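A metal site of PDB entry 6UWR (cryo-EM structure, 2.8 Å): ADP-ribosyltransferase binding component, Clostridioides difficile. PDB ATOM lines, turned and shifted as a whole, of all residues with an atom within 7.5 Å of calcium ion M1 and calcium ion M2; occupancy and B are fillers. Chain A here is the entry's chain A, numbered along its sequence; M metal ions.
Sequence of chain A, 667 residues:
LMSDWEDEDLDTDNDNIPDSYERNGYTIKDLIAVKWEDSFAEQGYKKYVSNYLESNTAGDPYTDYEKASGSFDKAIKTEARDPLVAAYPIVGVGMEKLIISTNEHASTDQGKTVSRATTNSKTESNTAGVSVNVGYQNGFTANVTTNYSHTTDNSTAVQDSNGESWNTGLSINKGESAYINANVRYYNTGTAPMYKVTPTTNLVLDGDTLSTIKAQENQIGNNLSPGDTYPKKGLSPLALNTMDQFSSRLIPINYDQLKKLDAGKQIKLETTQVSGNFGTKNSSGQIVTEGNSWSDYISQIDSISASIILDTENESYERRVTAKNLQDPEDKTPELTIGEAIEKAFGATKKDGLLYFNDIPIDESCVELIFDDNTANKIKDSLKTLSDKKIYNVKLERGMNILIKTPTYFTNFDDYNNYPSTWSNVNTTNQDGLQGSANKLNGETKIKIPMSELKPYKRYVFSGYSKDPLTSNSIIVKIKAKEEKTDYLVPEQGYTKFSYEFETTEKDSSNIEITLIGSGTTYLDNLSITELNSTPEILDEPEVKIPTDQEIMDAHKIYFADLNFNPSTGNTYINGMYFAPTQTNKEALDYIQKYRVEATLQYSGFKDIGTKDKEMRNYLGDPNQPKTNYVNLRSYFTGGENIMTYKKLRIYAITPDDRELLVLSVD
Of the 25 residues printed, 6 come within 4 Å of calcium ion M2. Along chain A the residues within 4 Å of calcium ion M2 span positions 13 to 64. The nearest printed residue that does not touch calcium ion M2 is Thr 57 (4.1 Å).
Calcium ion M2 is bound by OD2 of Asp 13, OD2 of Asp 64, O of Glu 54, O of Asn 51, OD2 of Asp 15, OE1 of Glu 22 and OE2 of Glu 22.
The side-chain carboxylate of Asp 64 is in hydrogen-bond range of the side-chain hydroxyl of Thr 57 (2.8 Å). The backbone NH (N) of Asp 64 lies within hydrogen-bond range of the backbone carbonyl oxygen (O) of Ser 55, at 2.9 Å. N of Asn 51 sits at hydrogen-bond distance from OG1 of Thr 57 (3.1 Å). OD1 of Asn 51 lies within hydrogen-bond range of N of Leu 53, at 3.0 Å. O of Asp 11 sits close to OD1 of Asn 14 (3.3 Å). O of Glu 22 is in hydrogen-bond range of N of Ser 50 (3.2 Å).
Of the 25 residues printed, 5 come within 4 Å of calcium ion M1.
Calcium ion M1 is bound by OD1 of Asp 13, 2.2 Å away. O of Ile 17 binds calcium ion M1. The side-chain carboxylate (OD1) of Asp 15 is bound to calcium ion M1, at 2.3 Å. OD1 of Asp 11 is bound to calcium ion M1, at 2.4 Å. The side-chain carboxylate (OE2) of Glu 22 binds calcium ion M1 (2.5 Å). Calcium ion M1 has five donor atoms within binding distance.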
ATOM      1  N   LEU A  10       9.488   1.597   1.232  1.00  0.00           N
ATOM      2  CA  LEU A  10       9.541   0.931  -0.062  1.00  0.00           C
ATOM      3  C   LEU A  10      10.135  -0.464   0.094  1.00  0.00           C
ATOM      4  O   LEU A  10      10.931  -0.725   0.995  1.00  0.00           O
ATOM      5  CB  LEU A  10      10.373   1.746  -1.045  1.00  0.00           C
ATOM      6  CG  LEU A  10       9.644   2.268  -2.272  1.00  0.00           C
ATOM      7  CD1 LEU A  10      10.620   2.967  -3.199  1.00  0.00           C
ATOM      8  CD2 LEU A  10       8.944   1.124  -2.992  1.00  0.00           C
ATOM      9  N   ASP A  11       9.725  -1.370  -0.798  1.00  0.00           N
ATOM     10  CA  ASP A  11      10.208  -2.748  -0.775  1.00  0.00           C
ATOM     11  C   ASP A  11      10.073  -3.294  -2.191  1.00  0.00           C
ATOM     12  O   ASP A  11       8.979  -3.702  -2.596  1.00  0.00           O
ATOM     13  CB  ASP A  11       9.417  -3.572   0.220  1.00  0.00           C
ATOM     14  CG  ASP A  11      10.281  -4.494   1.012  1.00  0.00           C
ATOM     15  OD1 ASP A  11      11.333  -4.927   0.501  1.00  0.00           O
ATOM     16  OD2 ASP A  11       9.909  -4.786   2.164  1.00  0.00           O
ATOM     17  N   THR A  12      11.174  -3.307  -2.932  1.00  0.00           N
ATOM     18  CA  THR A  12      11.091  -3.684  -4.336  1.00  0.00           C
ATOM     19  C   THR A  12      11.381  -5.169  -4.543  1.00  0.00           C
ATOM     20  O   THR A  12      10.822  -5.777  -5.449  1.00  0.00           O
ATOM     21  CB  THR A  12      12.053  -2.837  -5.159  1.00  0.00           C
ATOM     22  OG1 THR A  12      12.910  -2.113  -4.292  1.00  0.00           O
ATOM     23  CG2 THR A  12      11.280  -1.849  -5.986  1.00  0.00           C
ATOM     24  N   ASP A  13      12.258  -5.747  -3.734  1.00  0.00           N
ATOM     25  CA  ASP A  13      12.532  -7.169  -3.799  1.00  0.00           C
ATOM     26  C   ASP A  13      11.575  -7.989  -2.968  1.00  0.00           C
ATOM     27  O   ASP A  13      11.567  -9.212  -3.080  1.00  0.00           O
ATOM     28  CB  ASP A  13      13.973  -7.449  -3.354  1.00  0.00           C
ATOM     29  CG  ASP A  13      14.274  -6.917  -1.986  1.00  0.00           C
ATOM     30  OD1 ASP A  13      13.531  -6.053  -1.506  1.00  0.00           O
ATOM     31  OD2 ASP A  13      15.262  -7.367  -1.379  1.00  0.00           O
ATOM     32  N   ASN A  14      10.769  -7.337  -2.126  1.00  0.00           N
ATOM     33  CA  ASN A  14       9.650  -7.948  -1.431  1.00  0.00           C
ATOM     34  C   ASN A  14      10.077  -8.935  -0.360  1.00  0.00           C
ATOM     35  O   ASN A  14       9.299  -9.808   0.026  1.00  0.00           O
ATOM     36  CB  ASN A  14       8.680  -8.609  -2.407  1.00  0.00           C
ATOM     37  CG  ASN A  14       7.736  -7.627  -3.045  1.00  0.00           C
ATOM     38  OD1 ASN A  14       7.362  -6.626  -2.432  1.00  0.00           O
ATOM     39  ND2 ASN A  14       7.359  -7.884  -4.280  1.00  0.00           N
ATOM     40  N   ASP A  15      11.297  -8.834   0.149  1.00  0.00           N
ATOM     41  CA  ASP A  15      11.543  -9.370   1.476  1.00  0.00           C
ATOM     42  C   ASP A  15      11.013  -8.336   2.468  1.00  0.00           C
ATOM     43  O   ASP A  15      10.460  -7.303   2.087  1.00  0.00           O
ATOM     44  CB  ASP A  15      13.012  -9.709   1.687  1.00  0.00           C
ATOM     45  CG  ASP A  15      13.934  -8.674   1.123  1.00  0.00           C
ATOM     46  OD1 ASP A  15      13.522  -7.525   0.916  1.00  0.00           O
ATOM     47  OD2 ASP A  15      15.111  -9.012   0.883  1.00  0.00           O
ATOM     48  N   ASN A  16      11.143  -8.610   3.764  1.00  0.00           N
ATOM     49  CA  ASN A  16      10.525  -7.733   4.743  1.00  0.00           C
ATOM     50  C   ASN A  16      11.463  -6.638   5.234  1.00  0.00           C
ATOM     51  O   ASN A  16      11.288  -6.149   6.350  1.00  0.00           O
ATOM     52  CB  ASN A  16      10.015  -8.566   5.923  1.00  0.00           C
ATOM     53  CG  ASN A  16       9.068  -9.651   5.476  1.00  0.00           C
ATOM     54  OD1 ASN A  16       8.458  -9.560   4.420  1.00  0.00           O
ATOM     55  ND2 ASN A  16       8.952 -10.693   6.293  1.00  0.00           N
ATOM     56  N   ILE A  17      12.434  -6.251   4.427  1.00  0.00           N
ATOM     57  CA  ILE A  17      13.366  -5.169   4.767  1.00  0.00           C
ATOM     58  C   ILE A  17      13.162  -4.055   3.747  1.00  0.00           C
ATOM     59  O   ILE A  17      13.184  -4.313   2.545  1.00  0.00           O
ATOM     60  CB  ILE A  17      14.821  -5.656   4.756  1.00  0.00           C
ATOM     61  CG1 ILE A  17      14.933  -7.017   5.423  1.00  0.00           C
ATOM     62  CG2 ILE A  17      15.717  -4.658   5.435  1.00  0.00           C
ATOM     63  CD1 ILE A  17      16.232  -7.705   5.159  1.00  0.00           C
ATOM     64  N   PRO A  18      12.964  -2.816   4.186  1.00  0.00           N
ATOM     65  CA  PRO A  18      12.826  -1.714   3.232  1.00  0.00           C
ATOM     66  C   PRO A  18      14.134  -1.427   2.517  1.00  0.00           C
ATOM     67  O   PRO A  18      15.215  -1.829   2.928  1.00  0.00           O
ATOM     68  CB  PRO A  18      12.402  -0.537   4.120  1.00  0.00           C
ATOM     69  CG  PRO A  18      11.841  -1.159   5.334  1.00  0.00           C
ATOM     70  CD  PRO A  18      12.632  -2.398   5.556  1.00  0.00           C
ATOM     71  N   ASP A  19      14.017  -0.691   1.407  1.00  0.00           N
ATOM     72  CA  ASP A  19      15.188  -0.423   0.567  1.00  0.00           C
ATOM     73  C   ASP A  19      16.234   0.400   1.295  1.00  0.00           C
ATOM     74  O   ASP A  19      17.424   0.087   1.242  1.00  0.00           O
ATOM     75  CB  ASP A  19      14.756   0.292  -0.709  1.00  0.00           C
ATOM     76  CG  ASP A  19      13.764  -0.486  -1.512  1.00  0.00           C
ATOM     77  OD1 ASP A  19      13.278  -1.514  -1.003  1.00  0.00           O
ATOM     78  OD2 ASP A  19      13.451  -0.069  -2.640  1.00  0.00           O
ATOM     79  N   SER A  20      15.803   1.474   1.964  1.00  0.00           N
ATOM     80  CA  SER A  20      16.730   2.318   2.696  1.00  0.00           C
ATOM     81  C   SER A  20      17.484   1.562   3.776  1.00  0.00           C
ATOM     82  O   SER A  20      18.663   1.833   3.983  1.00  0.00           O
ATOM     83  CB  SER A  20      15.975   3.498   3.297  1.00  0.00           C
ATOM     84  OG  SER A  20      14.687   3.108   3.703  1.00  0.00           O
ATOM     85  N   GLU A  22      18.249  -1.657   3.667  1.00  0.00           N
ATOM     86  CA  GLU A  22      19.204  -2.525   3.010  1.00  0.00           C
ATOM     87  C   GLU A  22      20.407  -1.742   2.498  1.00  0.00           C
ATOM     88  O   GLU A  22      21.519  -2.268   2.491  1.00  0.00           O
ATOM     89  CB  GLU A  22      18.536  -3.260   1.856  1.00  0.00           C
ATOM     90  CG  GLU A  22      17.380  -4.105   2.282  1.00  0.00           C
ATOM     91  CD  GLU A  22      17.281  -5.380   1.496  1.00  0.00           C
ATOM     92  OE1 GLU A  22      18.297  -6.076   1.376  1.00  0.00           O
ATOM     93  OE2 GLU A  22      16.186  -5.695   1.003  1.00  0.00           O
ATOM     94  N   TYR A  26      20.917  -2.186   8.715  1.00  0.00           N
ATOM     95  CA  TYR A  26      19.792  -2.535   9.558  1.00  0.00           C
ATOM     96  C   TYR A  26      20.208  -3.648  10.508  1.00  0.00           C
ATOM     97  O   TYR A  26      21.325  -4.170  10.439  1.00  0.00           O
ATOM     98  CB  TYR A  26      18.581  -2.963   8.727  1.00  0.00           C
ATOM     99  CG  TYR A  26      18.822  -4.224   7.920  1.00  0.00           C
ATOM    100  CD1 TYR A  26      19.451  -4.166   6.698  1.00  0.00           C
ATOM    101  CD2 TYR A  26      18.416  -5.453   8.391  1.00  0.00           C
ATOM    102  CE1 TYR A  26      19.669  -5.305   5.966  1.00  0.00           C
ATOM    103  CE2 TYR A  26      18.641  -6.588   7.670  1.00  0.00           C
ATOM    104  CZ  TYR A  26      19.264  -6.512   6.463  1.00  0.00           C
ATOM    105  OH  TYR A  26      19.482  -7.651   5.731  1.00  0.00           O
ATOM    106  N   SER A  50      22.519  -5.327   2.443  1.00  0.00           N
ATOM    107  CA  SER A  50      22.188  -6.329   1.439  1.00  0.00           C
ATOM    108  C   SER A  50      21.689  -5.620   0.186  1.00  0.00           C
ATOM    109  O   SER A  50      21.690  -4.389   0.100  1.00  0.00           O
ATOM    110  CB  SER A  50      21.148  -7.310   1.973  1.00  0.00           C
ATOM    111  OG  SER A  50      20.194  -6.651   2.780  1.00  0.00           O
ATOM    112  N   ASN A  51      21.288  -6.411  -0.797  1.00  0.00           N
ATOM    113  CA  ASN A  51      20.831  -5.922  -2.078  1.00  0.00           C
ATOM    114  C   ASN A  51      19.334  -5.639  -1.993  1.00  0.00           C
ATOM    115  O   ASN A  51      18.551  -6.535  -1.699  1.00  0.00           O
ATOM    116  CB  ASN A  51      21.135  -6.933  -3.172  1.00  0.00           C
ATOM    117  CG  ASN A  51      20.966  -6.389  -4.562  1.00  0.00           C
ATOM    118  OD1 ASN A  51      20.321  -5.363  -4.756  1.00  0.00           O
ATOM    119  ND2 ASN A  51      21.526  -7.068  -5.532  1.00  0.00           N
ATOM    120  N   TYR A  52      18.947  -4.387  -2.231  1.00  0.00           N
ATOM    121  CA  TYR A  52      17.548  -4.016  -2.131  1.00  0.00           C
ATOM    122  C   TYR A  52      16.774  -4.309  -3.399  1.00  0.00           C
ATOM    123  O   TYR A  52      15.565  -4.071  -3.433  1.00  0.00           O
ATOM    124  CB  TYR A  52      17.417  -2.543  -1.754  1.00  0.00           C
ATOM    125  CG  TYR A  52      17.755  -1.589  -2.866  1.00  0.00           C
ATOM    126  CD1 TYR A  52      19.057  -1.231  -3.122  1.00  0.00           C
ATOM    127  CD2 TYR A  52      16.766  -1.037  -3.663  1.00  0.00           C
ATOM    128  CE1 TYR A  52      19.369  -0.356  -4.133  1.00  0.00           C
ATOM    129  CE2 TYR A  52      17.061  -0.176  -4.670  1.00  0.00           C
ATOM    130  CZ  TYR A  52      18.358   0.161  -4.902  1.00  0.00           C
ATOM    131  OH  TYR A  52      18.670   1.036  -5.913  1.00  0.00           O
ATOM    132  N   LEU A  53      17.440  -4.788  -4.437  1.00  0.00           N
ATOM    133  CA  LEU A  53      16.781  -5.245  -5.655  1.00  0.00           C
ATOM    134  C   LEU A  53      16.841  -6.756  -5.801  1.00  0.00           C
ATOM    135  O   LEU A  53      16.436  -7.295  -6.827  1.00  0.00           O
ATOM    136  CB  LEU A  53      17.420  -4.584  -6.881  1.00  0.00           C
ATOM    137  CG  LEU A  53      17.103  -3.116  -7.153  1.00  0.00           C
ATOM    138  CD1 LEU A  53      17.859  -2.675  -8.366  1.00  0.00           C
ATOM    139  CD2 LEU A  53      15.618  -2.932  -7.358  1.00  0.00           C
ATOM    140  N   GLU A  54      17.342  -7.453  -4.785  1.00  0.00           N
ATOM    141  CA  GLU A  54      17.511  -8.890  -4.803  1.00  0.00           C
ATOM    142  C   GLU A  54      16.941  -9.446  -3.508  1.00  0.00           C
ATOM    143  O   GLU A  54      17.283  -8.965  -2.432  1.00  0.00           O
ATOM    144  CB  GLU A  54      18.991  -9.258  -4.923  1.00  0.00           C
ATOM    145  CG  GLU A  54      19.248 -10.587  -5.581  1.00  0.00           C
ATOM    146  CD  GLU A  54      18.880 -10.597  -7.047  1.00  0.00           C
ATOM    147  OE1 GLU A  54      19.545  -9.899  -7.840  1.00  0.00           O
ATOM    148  OE2 GLU A  54      17.918 -11.310  -7.410  1.00  0.00           O
ATOM    149  N   SER A  55      16.084 -10.449  -3.619  1.00  0.00           N
ATOM    150  CA  SER A  55      15.519 -11.058  -2.422  1.00  0.00           C
ATOM    151  C   SER A  55      16.503 -12.001  -1.758  1.00  0.00           C
ATOM    152  O   SER A  55      16.451 -12.183  -0.540  1.00  0.00           O
ATOM    153  CB  SER A  55      14.225 -11.781  -2.762  1.00  0.00           C
ATOM    154  OG  SER A  55      13.500 -12.084  -1.600  1.00  0.00           O
ATOM    155  N   ASN A  56      17.392 -12.599  -2.544  1.00  0.00           N
ATOM    156  CA  ASN A  56      18.438 -13.495  -2.059  1.00  0.00           C
ATOM    157  C   ASN A  56      19.754 -12.893  -2.515  1.00  0.00           C
ATOM    158  O   ASN A  56      20.195 -13.132  -3.634  1.00  0.00           O
ATOM    159  CB  ASN A  56      18.265 -14.917  -2.601  1.00  0.00           C
ATOM    160  CG  ASN A  56      17.025 -15.602  -2.077  1.00  0.00           C
ATOM    161  OD1 ASN A  56      17.119 -16.587  -1.366  1.00  0.00           O
ATOM    162  ND2 ASN A  56      15.865 -15.090  -2.445  1.00  0.00           N
ATOM    163  N   THR A  57      20.379 -12.094  -1.652  1.00  0.00           N
ATOM    164  CA  THR A  57      21.585 -11.384  -2.048  1.00  0.00           C
ATOM    165  C   THR A  57      22.729 -12.349  -2.314  1.00  0.00           C
ATOM    166  O   THR A  57      23.423 -12.241  -3.337  1.00  0.00           O
ATOM    167  CB  THR A  57      21.982 -10.385  -0.963  1.00  0.00           C
ATOM    168  OG1 THR A  57      20.905  -9.473  -0.746  1.00  0.00           O
ATOM    169  CG2 THR A  57      23.212  -9.612  -1.380  1.00  0.00           C
ATOM    170  N   THR A  63      16.268 -16.154   1.877  1.00  0.00           N
ATOM    171  CA  THR A  63      16.167 -14.743   1.581  1.00  0.00           C
ATOM    172  C   THR A  63      16.958 -13.918   2.585  1.00  0.00           C
ATOM    173  O   THR A  63      17.402 -14.420   3.619  1.00  0.00           O
ATOM    174  CB  THR A  63      14.702 -14.286   1.572  1.00  0.00           C
ATOM    175  OG1 THR A  63      14.212 -14.231   2.904  1.00  0.00           O
ATOM    176  CG2 THR A  63      13.862 -15.244   0.786  1.00  0.00           C
ATOM    177  N   ASP A  64      17.139 -12.641   2.271  1.00  0.00           N
ATOM    178  CA  ASP A  64      17.897 -11.757   3.163  1.00  0.00           C
ATOM    179  C   ASP A  64      17.269 -11.692   4.546  1.00  0.00           C
ATOM    180  O   ASP A  64      18.001 -11.662   5.545  1.00  0.00           O
ATOM    181  CB  ASP A  64      17.979 -10.358   2.559  1.00  0.00           C
ATOM    182  CG  ASP A  64      18.878 -10.298   1.367  1.00  0.00           C
ATOM    183  OD1 ASP A  64      19.786 -11.135   1.268  1.00  0.00           O
ATOM    184  OD2 ASP A  64      18.694  -9.411   0.524  1.00  0.00           O
ATOM    185  N   TYR A  65      15.947 -11.681   4.623  1.00  0.00           N
ATOM    186  CA  TYR A  65      15.288 -11.623   5.917  1.00  0.00           C
ATOM    187  C   TYR A  65      15.466 -12.917   6.705  1.00  0.00           C
ATOM    188  O   TYR A  65      15.749 -12.881   7.898  1.00  0.00           O
ATOM    189  CB  TYR A  65      13.813 -11.300   5.764  1.00  0.00           C
ATOM    190  CG  TYR A  65      13.110 -11.230   7.088  1.00  0.00           C
ATOM    191  CD1 TYR A  65      13.215 -10.107   7.883  1.00  0.00           C
ATOM    192  CD2 TYR A  65      12.370 -12.297   7.558  1.00  0.00           C
ATOM    193  CE1 TYR A  65      12.600 -10.036   9.091  1.00  0.00           C
ATOM    194  CE2 TYR A  65      11.745 -12.234   8.773  1.00  0.00           C
ATOM    195  CZ  TYR A  65      11.861 -11.097   9.542  1.00  0.00           C
ATOM    196  OH  TYR A  65      11.237 -11.034  10.757  1.00  0.00           O
ATOM    197  N   PRO A  83      23.487 -11.321   5.137  1.00  0.00           N
ATOM    198  CA  PRO A  83      23.075 -11.590   3.759  1.00  0.00           C
ATOM    199  C   PRO A  83      24.213 -11.622   2.745  1.00  0.00           C
ATOM    200  O   PRO A  83      23.949 -11.866   1.568  1.00  0.00           O
ATOM    201  CB  PRO A  83      22.118 -10.441   3.461  1.00  0.00           C
ATOM    202  CG  PRO A  83      21.626 -10.022   4.772  1.00  0.00           C
ATOM    203  CD  PRO A  83      22.784 -10.155   5.688  1.00  0.00           C
HETATM  204 CA    CA M   1      13.756  -5.240   0.542  1.00  0.00          CA
HETATM  205 CA    CA M   2      17.178  -7.892  -0.346  1.00  0.00          CA
